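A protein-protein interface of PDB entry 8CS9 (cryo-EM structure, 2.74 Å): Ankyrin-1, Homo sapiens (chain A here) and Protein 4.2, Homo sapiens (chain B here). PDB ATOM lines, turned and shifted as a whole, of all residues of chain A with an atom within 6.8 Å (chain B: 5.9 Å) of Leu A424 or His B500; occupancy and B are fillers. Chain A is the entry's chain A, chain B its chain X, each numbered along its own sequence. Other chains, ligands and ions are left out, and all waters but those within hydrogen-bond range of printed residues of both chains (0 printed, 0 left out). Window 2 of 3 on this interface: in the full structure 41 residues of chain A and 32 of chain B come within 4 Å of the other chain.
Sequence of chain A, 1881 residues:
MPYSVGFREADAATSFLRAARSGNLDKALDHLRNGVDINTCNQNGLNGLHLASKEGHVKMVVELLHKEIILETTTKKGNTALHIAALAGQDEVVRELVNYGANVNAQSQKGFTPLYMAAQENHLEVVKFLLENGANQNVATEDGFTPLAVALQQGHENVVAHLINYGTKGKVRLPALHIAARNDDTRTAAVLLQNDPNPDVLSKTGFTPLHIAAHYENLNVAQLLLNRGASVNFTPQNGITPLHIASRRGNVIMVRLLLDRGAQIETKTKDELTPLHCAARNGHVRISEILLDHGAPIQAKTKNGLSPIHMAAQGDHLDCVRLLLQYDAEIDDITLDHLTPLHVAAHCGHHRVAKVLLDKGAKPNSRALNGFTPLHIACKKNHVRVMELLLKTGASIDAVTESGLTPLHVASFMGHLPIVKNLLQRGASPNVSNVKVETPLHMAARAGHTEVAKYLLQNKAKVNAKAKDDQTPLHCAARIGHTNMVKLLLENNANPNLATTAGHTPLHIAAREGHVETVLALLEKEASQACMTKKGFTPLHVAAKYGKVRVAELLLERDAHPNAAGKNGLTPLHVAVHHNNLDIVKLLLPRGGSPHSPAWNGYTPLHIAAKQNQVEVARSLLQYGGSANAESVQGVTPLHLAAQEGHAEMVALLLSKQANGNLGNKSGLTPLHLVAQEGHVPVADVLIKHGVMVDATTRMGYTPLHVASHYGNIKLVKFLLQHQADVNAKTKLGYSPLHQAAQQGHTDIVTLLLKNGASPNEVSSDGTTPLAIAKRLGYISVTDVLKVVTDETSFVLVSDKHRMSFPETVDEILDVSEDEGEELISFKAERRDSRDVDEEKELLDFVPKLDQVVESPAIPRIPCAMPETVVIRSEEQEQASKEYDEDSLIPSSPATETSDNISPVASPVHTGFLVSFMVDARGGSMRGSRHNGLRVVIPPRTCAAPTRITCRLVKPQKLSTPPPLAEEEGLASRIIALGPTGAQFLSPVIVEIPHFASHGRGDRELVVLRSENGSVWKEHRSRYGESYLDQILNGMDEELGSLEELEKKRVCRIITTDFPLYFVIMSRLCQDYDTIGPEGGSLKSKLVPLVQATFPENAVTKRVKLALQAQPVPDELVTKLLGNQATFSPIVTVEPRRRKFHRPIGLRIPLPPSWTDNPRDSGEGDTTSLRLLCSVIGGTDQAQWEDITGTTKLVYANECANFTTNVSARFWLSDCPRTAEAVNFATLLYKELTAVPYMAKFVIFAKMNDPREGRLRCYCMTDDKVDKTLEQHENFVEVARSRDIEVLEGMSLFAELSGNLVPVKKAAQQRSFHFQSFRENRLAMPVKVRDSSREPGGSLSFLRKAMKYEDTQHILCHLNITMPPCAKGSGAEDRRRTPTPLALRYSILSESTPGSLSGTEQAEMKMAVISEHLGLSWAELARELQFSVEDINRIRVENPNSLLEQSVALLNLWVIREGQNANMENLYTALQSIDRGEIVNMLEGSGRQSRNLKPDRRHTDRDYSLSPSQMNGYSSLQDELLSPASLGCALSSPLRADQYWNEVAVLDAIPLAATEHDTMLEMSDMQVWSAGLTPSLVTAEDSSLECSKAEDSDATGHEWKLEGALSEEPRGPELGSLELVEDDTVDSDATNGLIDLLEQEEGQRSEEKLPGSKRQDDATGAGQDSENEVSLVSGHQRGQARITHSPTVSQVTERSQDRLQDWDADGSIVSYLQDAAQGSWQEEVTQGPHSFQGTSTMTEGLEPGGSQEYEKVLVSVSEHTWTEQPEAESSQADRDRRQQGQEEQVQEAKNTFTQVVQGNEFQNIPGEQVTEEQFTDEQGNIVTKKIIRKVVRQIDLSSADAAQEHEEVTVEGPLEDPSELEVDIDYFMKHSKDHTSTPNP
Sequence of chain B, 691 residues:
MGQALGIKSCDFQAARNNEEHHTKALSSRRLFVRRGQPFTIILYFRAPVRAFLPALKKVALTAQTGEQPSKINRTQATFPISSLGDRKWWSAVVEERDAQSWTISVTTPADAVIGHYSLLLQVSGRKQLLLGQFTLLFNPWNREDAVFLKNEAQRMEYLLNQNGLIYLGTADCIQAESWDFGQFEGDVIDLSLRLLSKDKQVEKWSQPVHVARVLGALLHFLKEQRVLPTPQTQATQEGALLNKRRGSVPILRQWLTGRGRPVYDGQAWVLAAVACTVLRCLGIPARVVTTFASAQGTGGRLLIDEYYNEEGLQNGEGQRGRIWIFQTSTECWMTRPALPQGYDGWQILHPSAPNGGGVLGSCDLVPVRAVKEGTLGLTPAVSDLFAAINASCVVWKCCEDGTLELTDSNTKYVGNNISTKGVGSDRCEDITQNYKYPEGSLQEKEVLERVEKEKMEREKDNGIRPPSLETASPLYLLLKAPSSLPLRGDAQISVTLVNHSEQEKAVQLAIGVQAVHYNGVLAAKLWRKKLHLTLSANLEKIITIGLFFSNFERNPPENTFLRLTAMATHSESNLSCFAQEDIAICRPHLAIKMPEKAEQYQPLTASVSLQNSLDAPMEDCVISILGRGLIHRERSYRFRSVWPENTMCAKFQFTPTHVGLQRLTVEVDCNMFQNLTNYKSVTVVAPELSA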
ATOM      1  N   ILE A 397     -10.789 -11.193 -24.209  1.00  0.00           N
ATOM      2  CA  ILE A 397     -12.055 -10.525 -23.935  1.00  0.00           C
ATOM      3  C   ILE A 397     -12.638 -10.929 -22.587  1.00  0.00           C
ATOM      4  O   ILE A 397     -13.513 -10.229 -22.063  1.00  0.00           O
ATOM      5  CB  ILE A 397     -13.060 -10.807 -25.067  1.00  0.00           C
ATOM      6  CG1 ILE A 397     -14.085  -9.678 -25.176  1.00  0.00           C
ATOM      7  CG2 ILE A 397     -13.755 -12.145 -24.864  1.00  0.00           C
ATOM      8  CD1 ILE A 397     -15.059  -9.849 -26.311  1.00  0.00           C
ATOM      9  N   LEU A 408     -16.712  -6.386 -19.687  1.00  0.00           N
ATOM     10  CA  LEU A 408     -18.178  -6.087 -19.675  1.00  0.00           C
ATOM     11  C   LEU A 408     -18.627  -5.578 -18.296  1.00  0.00           C
ATOM     12  O   LEU A 408     -19.534  -4.767 -18.249  1.00  0.00           O
ATOM     13  CB  LEU A 408     -18.980  -7.305 -20.134  1.00  0.00           C
ATOM     14  CG  LEU A 408     -20.429  -7.038 -20.519  1.00  0.00           C
ATOM     15  CD1 LEU A 408     -20.508  -6.046 -21.662  1.00  0.00           C
ATOM     16  CD2 LEU A 408     -21.132  -8.331 -20.880  1.00  0.00           C
ATOM     17  N   SER A 412     -20.374  -2.041 -18.408  1.00  0.00           N
ATOM     18  CA  SER A 412     -21.744  -1.939 -17.921  1.00  0.00           C
ATOM     19  C   SER A 412     -21.833  -1.021 -16.711  1.00  0.00           C
ATOM     20  O   SER A 412     -22.832  -0.315 -16.538  1.00  0.00           O
ATOM     21  CB  SER A 412     -22.288  -3.325 -17.583  1.00  0.00           C
ATOM     22  OG  SER A 412     -22.522  -4.085 -18.755  1.00  0.00           O
ATOM     23  N   ILE A 419     -19.535   0.213 -26.151  1.00  0.00           N
ATOM     24  CA  ILE A 419     -18.610  -0.815 -25.685  1.00  0.00           C
ATOM     25  C   ILE A 419     -19.360  -2.082 -25.298  1.00  0.00           C
ATOM     26  O   ILE A 419     -18.935  -3.194 -25.627  1.00  0.00           O
ATOM     27  CB  ILE A 419     -17.764  -0.288 -24.514  1.00  0.00           C
ATOM     28  CG1 ILE A 419     -17.107   1.044 -24.883  1.00  0.00           C
ATOM     29  CG2 ILE A 419     -16.726  -1.313 -24.114  1.00  0.00           C
ATOM     30  CD1 ILE A 419     -15.839   0.898 -25.678  1.00  0.00           C
ATOM     31  N   VAL A 420     -20.478  -1.935 -24.585  1.00  0.00           N
ATOM     32  CA  VAL A 420     -21.258  -3.092 -24.155  1.00  0.00           C
ATOM     33  C   VAL A 420     -21.809  -3.842 -25.362  1.00  0.00           C
ATOM     34  O   VAL A 420     -21.737  -5.076 -25.432  1.00  0.00           O
ATOM     35  CB  VAL A 420     -22.374  -2.636 -23.196  1.00  0.00           C
ATOM     36  CG1 VAL A 420     -23.491  -3.656 -23.129  1.00  0.00           C
ATOM     37  CG2 VAL A 420     -21.809  -2.376 -21.816  1.00  0.00           C
ATOM     38  N   LYS A 421     -22.346  -3.106 -26.337  1.00  0.00           N
ATOM     39  CA  LYS A 421     -22.872  -3.721 -27.549  1.00  0.00           C
ATOM     40  C   LYS A 421     -21.778  -4.433 -28.335  1.00  0.00           C
ATOM     41  O   LYS A 421     -21.983  -5.552 -28.817  1.00  0.00           O
ATOM     42  CB  LYS A 421     -23.551  -2.657 -28.411  1.00  0.00           C
ATOM     43  CG  LYS A 421     -24.151  -3.173 -29.702  1.00  0.00           C
ATOM     44  CD  LYS A 421     -24.909  -2.075 -30.433  1.00  0.00           C
ATOM     45  CE  LYS A 421     -26.207  -1.726 -29.723  1.00  0.00           C
ATOM     46  NZ  LYS A 421     -26.099  -0.463 -28.938  1.00  0.00           N
ATOM     47  N   ASN A 422     -20.605  -3.806 -28.469  1.00  0.00           N
ATOM     48  CA  ASN A 422     -19.517  -4.425 -29.216  1.00  0.00           C
ATOM     49  C   ASN A 422     -19.000  -5.673 -28.513  1.00  0.00           C
ATOM     50  O   ASN A 422     -18.734  -6.692 -29.159  1.00  0.00           O
ATOM     51  CB  ASN A 422     -18.388  -3.418 -29.425  1.00  0.00           C
ATOM     52  CG  ASN A 422     -17.798  -3.485 -30.818  1.00  0.00           C
ATOM     53  OD1 ASN A 422     -17.121  -4.448 -31.174  1.00  0.00           O
ATOM     54  ND2 ASN A 422     -18.052  -2.456 -31.618  1.00  0.00           N
ATOM     55  N   LEU A 423     -18.847  -5.613 -27.186  1.00  0.00           N
ATOM     56  CA  LEU A 423     -18.403  -6.775 -26.429  1.00  0.00           C
ATOM     57  C   LEU A 423     -19.392  -7.927 -26.504  1.00  0.00           C
ATOM     58  O   LEU A 423     -18.970  -9.077 -26.651  1.00  0.00           O
ATOM     59  CB  LEU A 423     -18.169  -6.396 -24.966  1.00  0.00           C
ATOM     60  CG  LEU A 423     -16.923  -5.571 -24.639  1.00  0.00           C
ATOM     61  CD1 LEU A 423     -16.916  -5.175 -23.174  1.00  0.00           C
ATOM     62  CD2 LEU A 423     -15.660  -6.328 -24.997  1.00  0.00           C
ATOM     63  N   LEU A 424     -20.691  -7.650 -26.418  1.00  0.00           N
ATOM     64  CA  LEU A 424     -21.679  -8.717 -26.495  1.00  0.00           C
ATOM     65  C   LEU A 424     -21.854  -9.259 -27.905  1.00  0.00           C
ATOM     66  O   LEU A 424     -22.208 -10.432 -28.066  1.00  0.00           O
ATOM     67  CB  LEU A 424     -23.025  -8.231 -25.956  1.00  0.00           C
ATOM     68  CG  LEU A 424     -23.123  -8.158 -24.432  1.00  0.00           C
ATOM     69  CD1 LEU A 424     -24.137  -7.136 -23.997  1.00  0.00           C
ATOM     70  CD2 LEU A 424     -23.463  -9.512 -23.856  1.00  0.00           C
ATOM     71  N   GLN A 425     -21.625  -8.434 -28.929  1.00  0.00           N
ATOM     72  CA  GLN A 425     -21.678  -8.932 -30.298  1.00  0.00           C
ATOM     73  C   GLN A 425     -20.538  -9.904 -30.575  1.00  0.00           C
ATOM     74  O   GLN A 425     -20.719 -10.899 -31.284  1.00  0.00           O
ATOM     75  CB  GLN A 425     -21.642  -7.766 -31.283  1.00  0.00           C
ATOM     76  CG  GLN A 425     -23.008  -7.212 -31.636  1.00  0.00           C
ATOM     77  CD  GLN A 425     -22.938  -5.796 -32.172  1.00  0.00           C
ATOM     78  OE1 GLN A 425     -21.871  -5.187 -32.213  1.00  0.00           O
ATOM     79  NE2 GLN A 425     -24.082  -5.263 -32.588  1.00  0.00           N
ATOM     80  N   ARG A 426     -19.357  -9.635 -30.019  1.00  0.00           N
ATOM     81  CA  ARG A 426     -18.192 -10.478 -30.250  1.00  0.00           C
ATOM     82  C   ARG A 426     -18.204 -11.757 -29.423  1.00  0.00           C
ATOM     83  O   ARG A 426     -17.379 -12.641 -29.675  1.00  0.00           O
ATOM     84  CB  ARG A 426     -16.912  -9.691 -29.964  1.00  0.00           C
ATOM     85  CG  ARG A 426     -16.552  -8.709 -31.057  1.00  0.00           C
ATOM     86  CD  ARG A 426     -15.913  -7.448 -30.490  1.00  0.00           C
ATOM     87  NE  ARG A 426     -15.210  -6.645 -31.487  1.00  0.00           N
ATOM     88  CZ  ARG A 426     -14.188  -7.056 -32.226  1.00  0.00           C
ATOM     89  NH1 ARG A 426     -13.645  -8.253 -32.063  1.00  0.00           N
ATOM     90  NH2 ARG A 426     -13.683  -6.237 -33.141  1.00  0.00           N
ATOM     91  N   GLY A 427     -19.104 -11.879 -28.451  1.00  0.00           N
ATOM     92  CA  GLY A 427     -19.239 -13.116 -27.710  1.00  0.00           C
ATOM     93  C   GLY A 427     -18.663 -13.085 -26.310  1.00  0.00           C
ATOM     94  O   GLY A 427     -18.152 -14.098 -25.827  1.00  0.00           O
ATOM     95  N   ALA A 428     -18.726 -11.933 -25.651  1.00  0.00           N
ATOM     96  CA  ALA A 428     -18.346 -11.835 -24.251  1.00  0.00           C
ATOM     97  C   ALA A 428     -19.464 -12.397 -23.387  1.00  0.00           C
ATOM     98  O   ALA A 428     -20.644 -12.135 -23.634  1.00  0.00           O
ATOM     99  CB  ALA A 428     -18.054 -10.387 -23.858  1.00  0.00           C
ATOM    100  N   SER A 429     -19.088 -13.177 -22.379  1.00  0.00           N
ATOM    101  CA  SER A 429     -20.077 -13.826 -21.531  1.00  0.00           C
ATOM    102  C   SER A 429     -20.745 -12.792 -20.634  1.00  0.00           C
ATOM    103  O   SER A 429     -20.054 -12.114 -19.865  1.00  0.00           O
ATOM    104  CB  SER A 429     -19.436 -14.916 -20.686  1.00  0.00           C
ATOM    105  OG  SER A 429     -20.380 -15.480 -19.793  1.00  0.00           O
ATOM    106  N   PRO A 430     -22.066 -12.635 -20.701  1.00  0.00           N
ATOM    107  CA  PRO A 430     -22.759 -11.647 -19.871  1.00  0.00           C
ATOM    108  C   PRO A 430     -23.155 -12.140 -18.489  1.00  0.00           C
ATOM    109  O   PRO A 430     -23.806 -11.394 -17.753  1.00  0.00           O
ATOM    110  CB  PRO A 430     -24.007 -11.343 -20.712  1.00  0.00           C
ATOM    111  CG  PRO A 430     -24.273 -12.643 -21.399  1.00  0.00           C
ATOM    112  CD  PRO A 430     -22.950 -13.238 -21.712  1.00  0.00           C
ATOM    113  N   VAL A 452     -27.979   0.197 -21.138  1.00  0.00           N
ATOM    114  CA  VAL A 452     -27.011  -0.895 -21.064  1.00  0.00           C
ATOM    115  C   VAL A 452     -27.678  -2.152 -20.521  1.00  0.00           C
ATOM    116  O   VAL A 452     -27.493  -3.255 -21.048  1.00  0.00           O
ATOM    117  CB  VAL A 452     -25.800  -0.489 -20.207  1.00  0.00           C
ATOM    118  CG1 VAL A 452     -24.926  -1.696 -19.917  1.00  0.00           C
ATOM    119  CG2 VAL A 452     -24.999   0.596 -20.902  1.00  0.00           C
ATOM    120  N   TYR A 455     -29.958  -3.678 -23.136  1.00  0.00           N
ATOM    121  CA  TYR A 455     -29.224  -4.480 -24.107  1.00  0.00           C
ATOM    122  C   TYR A 455     -28.691  -5.765 -23.490  1.00  0.00           C
ATOM    123  O   TYR A 455     -28.570  -6.782 -24.181  1.00  0.00           O
ATOM    124  CB  TYR A 455     -28.081  -3.666 -24.713  1.00  0.00           C
ATOM    125  CG  TYR A 455     -27.412  -4.365 -25.868  1.00  0.00           C
ATOM    126  CD1 TYR A 455     -27.919  -4.265 -27.153  1.00  0.00           C
ATOM    127  CD2 TYR A 455     -26.276  -5.126 -25.677  1.00  0.00           C
ATOM    128  CE1 TYR A 455     -27.313  -4.910 -28.211  1.00  0.00           C
ATOM    129  CE2 TYR A 455     -25.662  -5.772 -26.730  1.00  0.00           C
ATOM    130  CZ  TYR A 455     -26.184  -5.664 -27.993  1.00  0.00           C
ATOM    131  OH  TYR A 455     -25.575  -6.308 -29.044  1.00  0.00           O
ATOM    132  N   LEU A 456     -28.341  -5.733 -22.204  1.00  0.00           N
ATOM    133  CA  LEU A 456     -27.901  -6.953 -21.535  1.00  0.00           C
ATOM    134  C   LEU A 456     -29.024  -7.976 -21.472  1.00  0.00           C
ATOM    135  O   LEU A 456     -28.784  -9.180 -21.619  1.00  0.00           O
ATOM    136  CB  LEU A 456     -27.389  -6.627 -20.133  1.00  0.00           C
ATOM    137  CG  LEU A 456     -25.973  -6.063 -20.015  1.00  0.00           C
ATOM    138  CD1 LEU A 456     -25.717  -5.563 -18.608  1.00  0.00           C
ATOM    139  CD2 LEU A 456     -24.944  -7.104 -20.397  1.00  0.00           C
ATOM    140  N   LEU A 457     -30.259  -7.514 -21.273  1.00  0.00           N
ATOM    141  CA  LEU A 457     -31.384  -8.430 -21.137  1.00  0.00           C
ATOM    142  C   LEU A 457     -31.876  -8.932 -22.492  1.00  0.00           C
ATOM    143  O   LEU A 457     -32.490 -10.002 -22.574  1.00  0.00           O
ATOM    144  CB  LEU A 457     -32.515  -7.755 -20.364  1.00  0.00           C
ATOM    145  CG  LEU A 457     -32.224  -7.472 -18.889  1.00  0.00           C
ATOM    146  CD1 LEU A 457     -33.049  -6.300 -18.395  1.00  0.00           C
ATOM    147  CD2 LEU A 457     -32.480  -8.707 -18.039  1.00  0.00           C
ATOM    148  N   ASN A 459     -29.819  -9.836 -24.879  1.00  0.00           N
ATOM    149  CA  ASN A 459     -28.949 -10.999 -24.931  1.00  0.00           C
ATOM    150  C   ASN A 459     -29.172 -11.827 -23.674  1.00  0.00           C
ATOM    151  O   ASN A 459     -30.115 -11.570 -22.920  1.00  0.00           O
ATOM    152  CB  ASN A 459     -27.489 -10.570 -25.065  1.00  0.00           C
ATOM    153  CG  ASN A 459     -27.289  -9.545 -26.161  1.00  0.00           C
ATOM    154  OD1 ASN A 459     -28.057  -9.482 -27.120  1.00  0.00           O
ATOM    155  ND2 ASN A 459     -26.263  -8.730 -26.018  1.00  0.00           N
ATOM    156  N   LYS A 460     -28.332 -12.825 -23.438  1.00  0.00           N
ATOM    157  CA  LYS A 460     -28.440 -13.640 -22.240  1.00  0.00           C
ATOM    158  C   LYS A 460     -28.148 -12.789 -21.013  1.00  0.00           C
ATOM    159  O   LYS A 460     -27.195 -12.009 -20.991  1.00  0.00           O
ATOM    160  CB  LYS A 460     -27.489 -14.837 -22.291  1.00  0.00           C
ATOM    161  CG  LYS A 460     -28.031 -16.009 -23.090  1.00  0.00           C
ATOM    162  CD  LYS A 460     -27.704 -15.870 -24.564  1.00  0.00           C
ATOM    163  CE  LYS A 460     -28.868 -16.316 -25.426  1.00  0.00           C
ATOM    164  NZ  LYS A 460     -28.485 -16.401 -26.860  1.00  0.00           N
ATOM    165  N   SER B 473     -29.307  -8.142 -36.611  1.00  0.00           N
ATOM    166  CA  SER B 473     -29.370  -8.038 -35.156  1.00  0.00           C
ATOM    167  C   SER B 473     -29.072  -9.369 -34.434  1.00  0.00           C
ATOM    168  O   SER B 473     -28.283  -9.374 -33.489  1.00  0.00           O
ATOM    169  CB  SER B 473     -30.731  -7.476 -34.716  1.00  0.00           C
ATOM    170  OG  SER B 473     -30.636  -6.820 -33.465  1.00  0.00           O
ATOM    171  N   PRO B 474     -29.670 -10.497 -34.853  1.00  0.00           N
ATOM    172  CA  PRO B 474     -29.236 -11.781 -34.285  1.00  0.00           C
ATOM    173  C   PRO B 474     -27.916 -12.269 -34.847  1.00  0.00           C
ATOM    174  O   PRO B 474     -27.357 -13.240 -34.320  1.00  0.00           O
ATOM    175  CB  PRO B 474     -30.379 -12.727 -34.661  1.00  0.00           C
ATOM    176  CG  PRO B 474     -30.812 -12.208 -35.963  1.00  0.00           C
ATOM    177  CD  PRO B 474     -30.809 -10.715 -35.771  1.00  0.00           C
ATOM    178  N   LEU B 475     -27.408 -11.630 -35.895  1.00  0.00           N
ATOM    179  CA  LEU B 475     -26.180 -12.024 -36.562  1.00  0.00           C
ATOM    180  C   LEU B 475     -25.161 -10.904 -36.408  1.00  0.00           C
ATOM    181  O   LEU B 475     -25.517  -9.724 -36.445  1.00  0.00           O
ATOM    182  CB  LEU B 475     -26.445 -12.315 -38.045  1.00  0.00           C
ATOM    183  CG  LEU B 475     -25.336 -12.829 -38.966  1.00  0.00           C
ATOM    184  CD1 LEU B 475     -24.372 -13.747 -38.233  1.00  0.00           C
ATOM    185  CD2 LEU B 475     -25.943 -13.540 -40.164  1.00  0.00           C
ATOM    186  N   TYR B 476     -23.900 -11.272 -36.206  1.00  0.00           N
ATOM    187  CA  TYR B 476     -22.802 -10.318 -36.148  1.00  0.00           C
ATOM    188  C   TYR B 476     -21.787 -10.670 -37.224  1.00  0.00           C
ATOM    189  O   TYR B 476     -21.440 -11.842 -37.394  1.00  0.00           O
ATOM    190  CB  TYR B 476     -22.140 -10.314 -34.771  1.00  0.00           C
ATOM    191  CG  TYR B 476     -20.903  -9.449 -34.684  1.00  0.00           C
ATOM    192  CD1 TYR B 476     -20.970  -8.083 -34.923  1.00  0.00           C
ATOM    193  CD2 TYR B 476     -19.670  -9.995 -34.358  1.00  0.00           C
ATOM    194  CE1 TYR B 476     -19.844  -7.288 -34.845  1.00  0.00           C
ATOM    195  CE2 TYR B 476     -18.538  -9.206 -34.275  1.00  0.00           C
ATOM    196  CZ  TYR B 476     -18.632  -7.855 -34.521  1.00  0.00           C
ATOM    197  OH  TYR B 476     -17.509  -7.068 -34.440  1.00  0.00           O
ATOM    198  N   VAL B 498     -21.094 -14.578 -36.291  1.00  0.00           N
ATOM    199  CA  VAL B 498     -21.483 -15.075 -34.976  1.00  0.00           C
ATOM    200  C   VAL B 498     -23.002 -15.138 -34.920  1.00  0.00           C
ATOM    201  O   VAL B 498     -23.678 -14.112 -35.061  1.00  0.00           O
ATOM    202  CB  VAL B 498     -20.931 -14.193 -33.844  1.00  0.00           C
ATOM    203  CG1 VAL B 498     -21.130 -14.873 -32.503  1.00  0.00           C
ATOM    204  CG2 VAL B 498     -19.460 -13.890 -34.075  1.00  0.00           C
ATOM    205  N   ASN B 499     -23.534 -16.336 -34.704  1.00  0.00           N
ATOM    206  CA  ASN B 499     -24.966 -16.553 -34.555  1.00  0.00           C
ATOM    207  C   ASN B 499     -25.318 -16.373 -33.083  1.00  0.00           C
ATOM    208  O   ASN B 499     -24.715 -17.014 -32.217  1.00  0.00           O
ATOM    209  CB  ASN B 499     -25.353 -17.951 -35.040  1.00  0.00           C
ATOM    210  CG  ASN B 499     -26.840 -18.096 -35.325  1.00  0.00           C
ATOM    211  OD1 ASN B 499     -27.644 -17.292 -34.864  1.00  0.00           O
ATOM    212  ND2 ASN B 499     -27.213 -19.127 -36.067  1.00  0.00           N
ATOM    213  N   HIS B 500     -26.280 -15.498 -32.802  1.00  0.00           N
ATOM    214  CA  HIS B 500     -26.767 -15.301 -31.445  1.00  0.00           C
ATOM    215  C   HIS B 500     -28.168 -15.854 -31.232  1.00  0.00           C
ATOM    216  O   HIS B 500     -28.654 -15.853 -30.096  1.00  0.00           O
ATOM    217  CB  HIS B 500     -26.737 -13.814 -31.083  1.00  0.00           C
ATOM    218  CG  HIS B 500     -25.364 -13.222 -31.086  1.00  0.00           C
ATOM    219  ND1 HIS B 500     -24.902 -12.416 -32.105  1.00  0.00           N
ATOM    220  CD2 HIS B 500     -24.344 -13.330 -30.202  1.00  0.00           C
ATOM    221  CE1 HIS B 500     -23.661 -12.048 -31.844  1.00  0.00           C
ATOM    222  NE2 HIS B 500     -23.298 -12.591 -30.696  1.00  0.00           N
ATOM    223  N   SER B 501     -28.823 -16.328 -32.286  1.00  0.00           N
ATOM    224  CA  SER B 501     -30.144 -16.920 -32.167  1.00  0.00           C
ATOM    225  C   SER B 501     -30.051 -18.333 -31.597  1.00  0.00           C
ATOM    226  O   SER B 501     -29.005 -18.986 -31.643  1.00  0.00           O
ATOM    227  CB  SER B 501     -30.846 -16.950 -33.525  1.00  0.00           C
ATOM    228  OG  SER B 501     -30.734 -18.228 -34.127  1.00  0.00           O
ATOM    229  N   GLU B 502     -31.171 -18.800 -31.048  1.00  0.00           N
ATOM    230  CA  GLU B 502     -31.254 -20.153 -30.515  1.00  0.00           C
ATOM    231  C   GLU B 502     -31.427 -21.207 -31.600  1.00  0.00           C
ATOM    232  O   GLU B 502     -31.287 -22.399 -31.309  1.00  0.00           O
ATOM    233  CB  GLU B 502     -32.409 -20.257 -29.517  1.00  0.00           C
ATOM    234  CG  GLU B 502     -32.111 -19.659 -28.153  1.00  0.00           C
ATOM    235  CD  GLU B 502     -30.795 -20.141 -27.578  1.00  0.00           C
ATOM    236  OE1 GLU B 502     -30.756 -21.269 -27.044  1.00  0.00           O
ATOM    237  OE2 GLU B 502     -29.801 -19.388 -27.652  1.00  0.00           O
ATOM    238  N   LYS B 505     -29.133 -20.894 -38.645  1.00  0.00           N
ATOM    239  CA  LYS B 505     -29.473 -19.884 -39.636  1.00  0.00           C
ATOM    240  C   LYS B 505     -28.929 -20.271 -41.003  1.00  0.00           C
ATOM    241  O   LYS B 505     -27.779 -20.704 -41.126  1.00  0.00           O
ATOM    242  CB  LYS B 505     -28.920 -18.518 -39.230  1.00  0.00           C
ATOM    243  CG  LYS B 505     -29.978 -17.460 -38.992  1.00  0.00           C
ATOM    244  CD  LYS B 505     -30.748 -17.736 -37.715  1.00  0.00           C
ATOM    245  CE  LYS B 505     -31.496 -16.502 -37.252  1.00  0.00           C
ATOM    246  NZ  LYS B 505     -30.563 -15.464 -36.748  1.00  0.00           N
ATOM    247  N   ASN B 538     -25.510 -20.280 -31.512  1.00  0.00           N
ATOM    248  CA  ASN B 538     -24.493 -19.804 -30.571  1.00  0.00           C
ATOM    249  C   ASN B 538     -23.095 -20.279 -30.960  1.00  0.00           C
ATOM    250  O   ASN B 538     -22.272 -20.608 -30.106  1.00  0.00           O
ATOM    251  CB  ASN B 538     -24.827 -20.220 -29.135  1.00  0.00           C
ATOM    252  CG  ASN B 538     -25.875 -19.334 -28.506  1.00  0.00           C
ATOM    253  OD1 ASN B 538     -27.038 -19.720 -28.384  1.00  0.00           O
ATOM    254  ND2 ASN B 538     -25.472 -18.135 -28.102  1.00  0.00           N
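Leu A424 touches just one residue of chain B: His B500.
His B500 touches just these residues of chain A: Leu A424 (3.6 Å), Gln A425 (3.1 Å) and Lys A460 (3.3 Å).
Printed residues of chain A within 4 Å of Glu B502: Lys A460 (3.4 Å).
Of the printed residues of chain A, Tyr B476 touches Gln A425 (3.4 Å) and Arg A426 (3.8 Å).
Asn A422 touches none of the printed residues of chain B.
The nearest printed residue of chain B that does not touch Leu A424 is Val B498 (6.4 Å).
The nearest residue of chain A that does not touch His B500 is Gly A427 (4.8 Å).
The nearest printed residue of chain A that does not touch Asn B538 is Gly A427 (8.0 Å).
Of the 21 printed residues of chain A, 4 touch a printed residue of chain B.
Among the printed residues, merely in contact across the chains: Leu A424 with His B500 (3.6 Å), Gln A425 with Tyr B476 (3.4 Å), Arg A426 with Tyr B476 (3.8 Å) and Lys A460 with Asn B538 (3.7 Å).
The side-chain amide oxygen (OD1) of Asn A422 lies within hydrogen-bond range of the guanidinium group (NE) of Arg A426 (2.9 Å).
OE2 of Glu B502 lies close to OD1 of Asn B538, 2.9 Å away.
The backbone carbonyl oxygen (O) of Lys A421 lies close to the side-chain amide oxygen (OE1) of Gln A425, 3.4 Å away.
The backbone carbonyl oxygen (O) of Tyr B476 is in hydrogen-bond range of the backbone NH (N) of Val B498, at 3.0 Å.
The backbone carbonyl oxygen (O) of Pro B474 sits at hydrogen-bond distance from the backbone NH (N) of His B500 (2.9 Å).
N of Asn B538 lies close to O of Asn B499 (3.4 Å).
The backbone carbonyl oxygen of Gln A425 sits at hydrogen-bond distance from a ring nitrogen (NE2) of His B500 (3.1 Å).
NZ of Lys A460 sits at hydrogen-bond distance from O of His B500, at 3.3 Å.
OE2 of Glu B502 lies within salt-bridge range of NZ of Lys A460 (3.4 Å).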
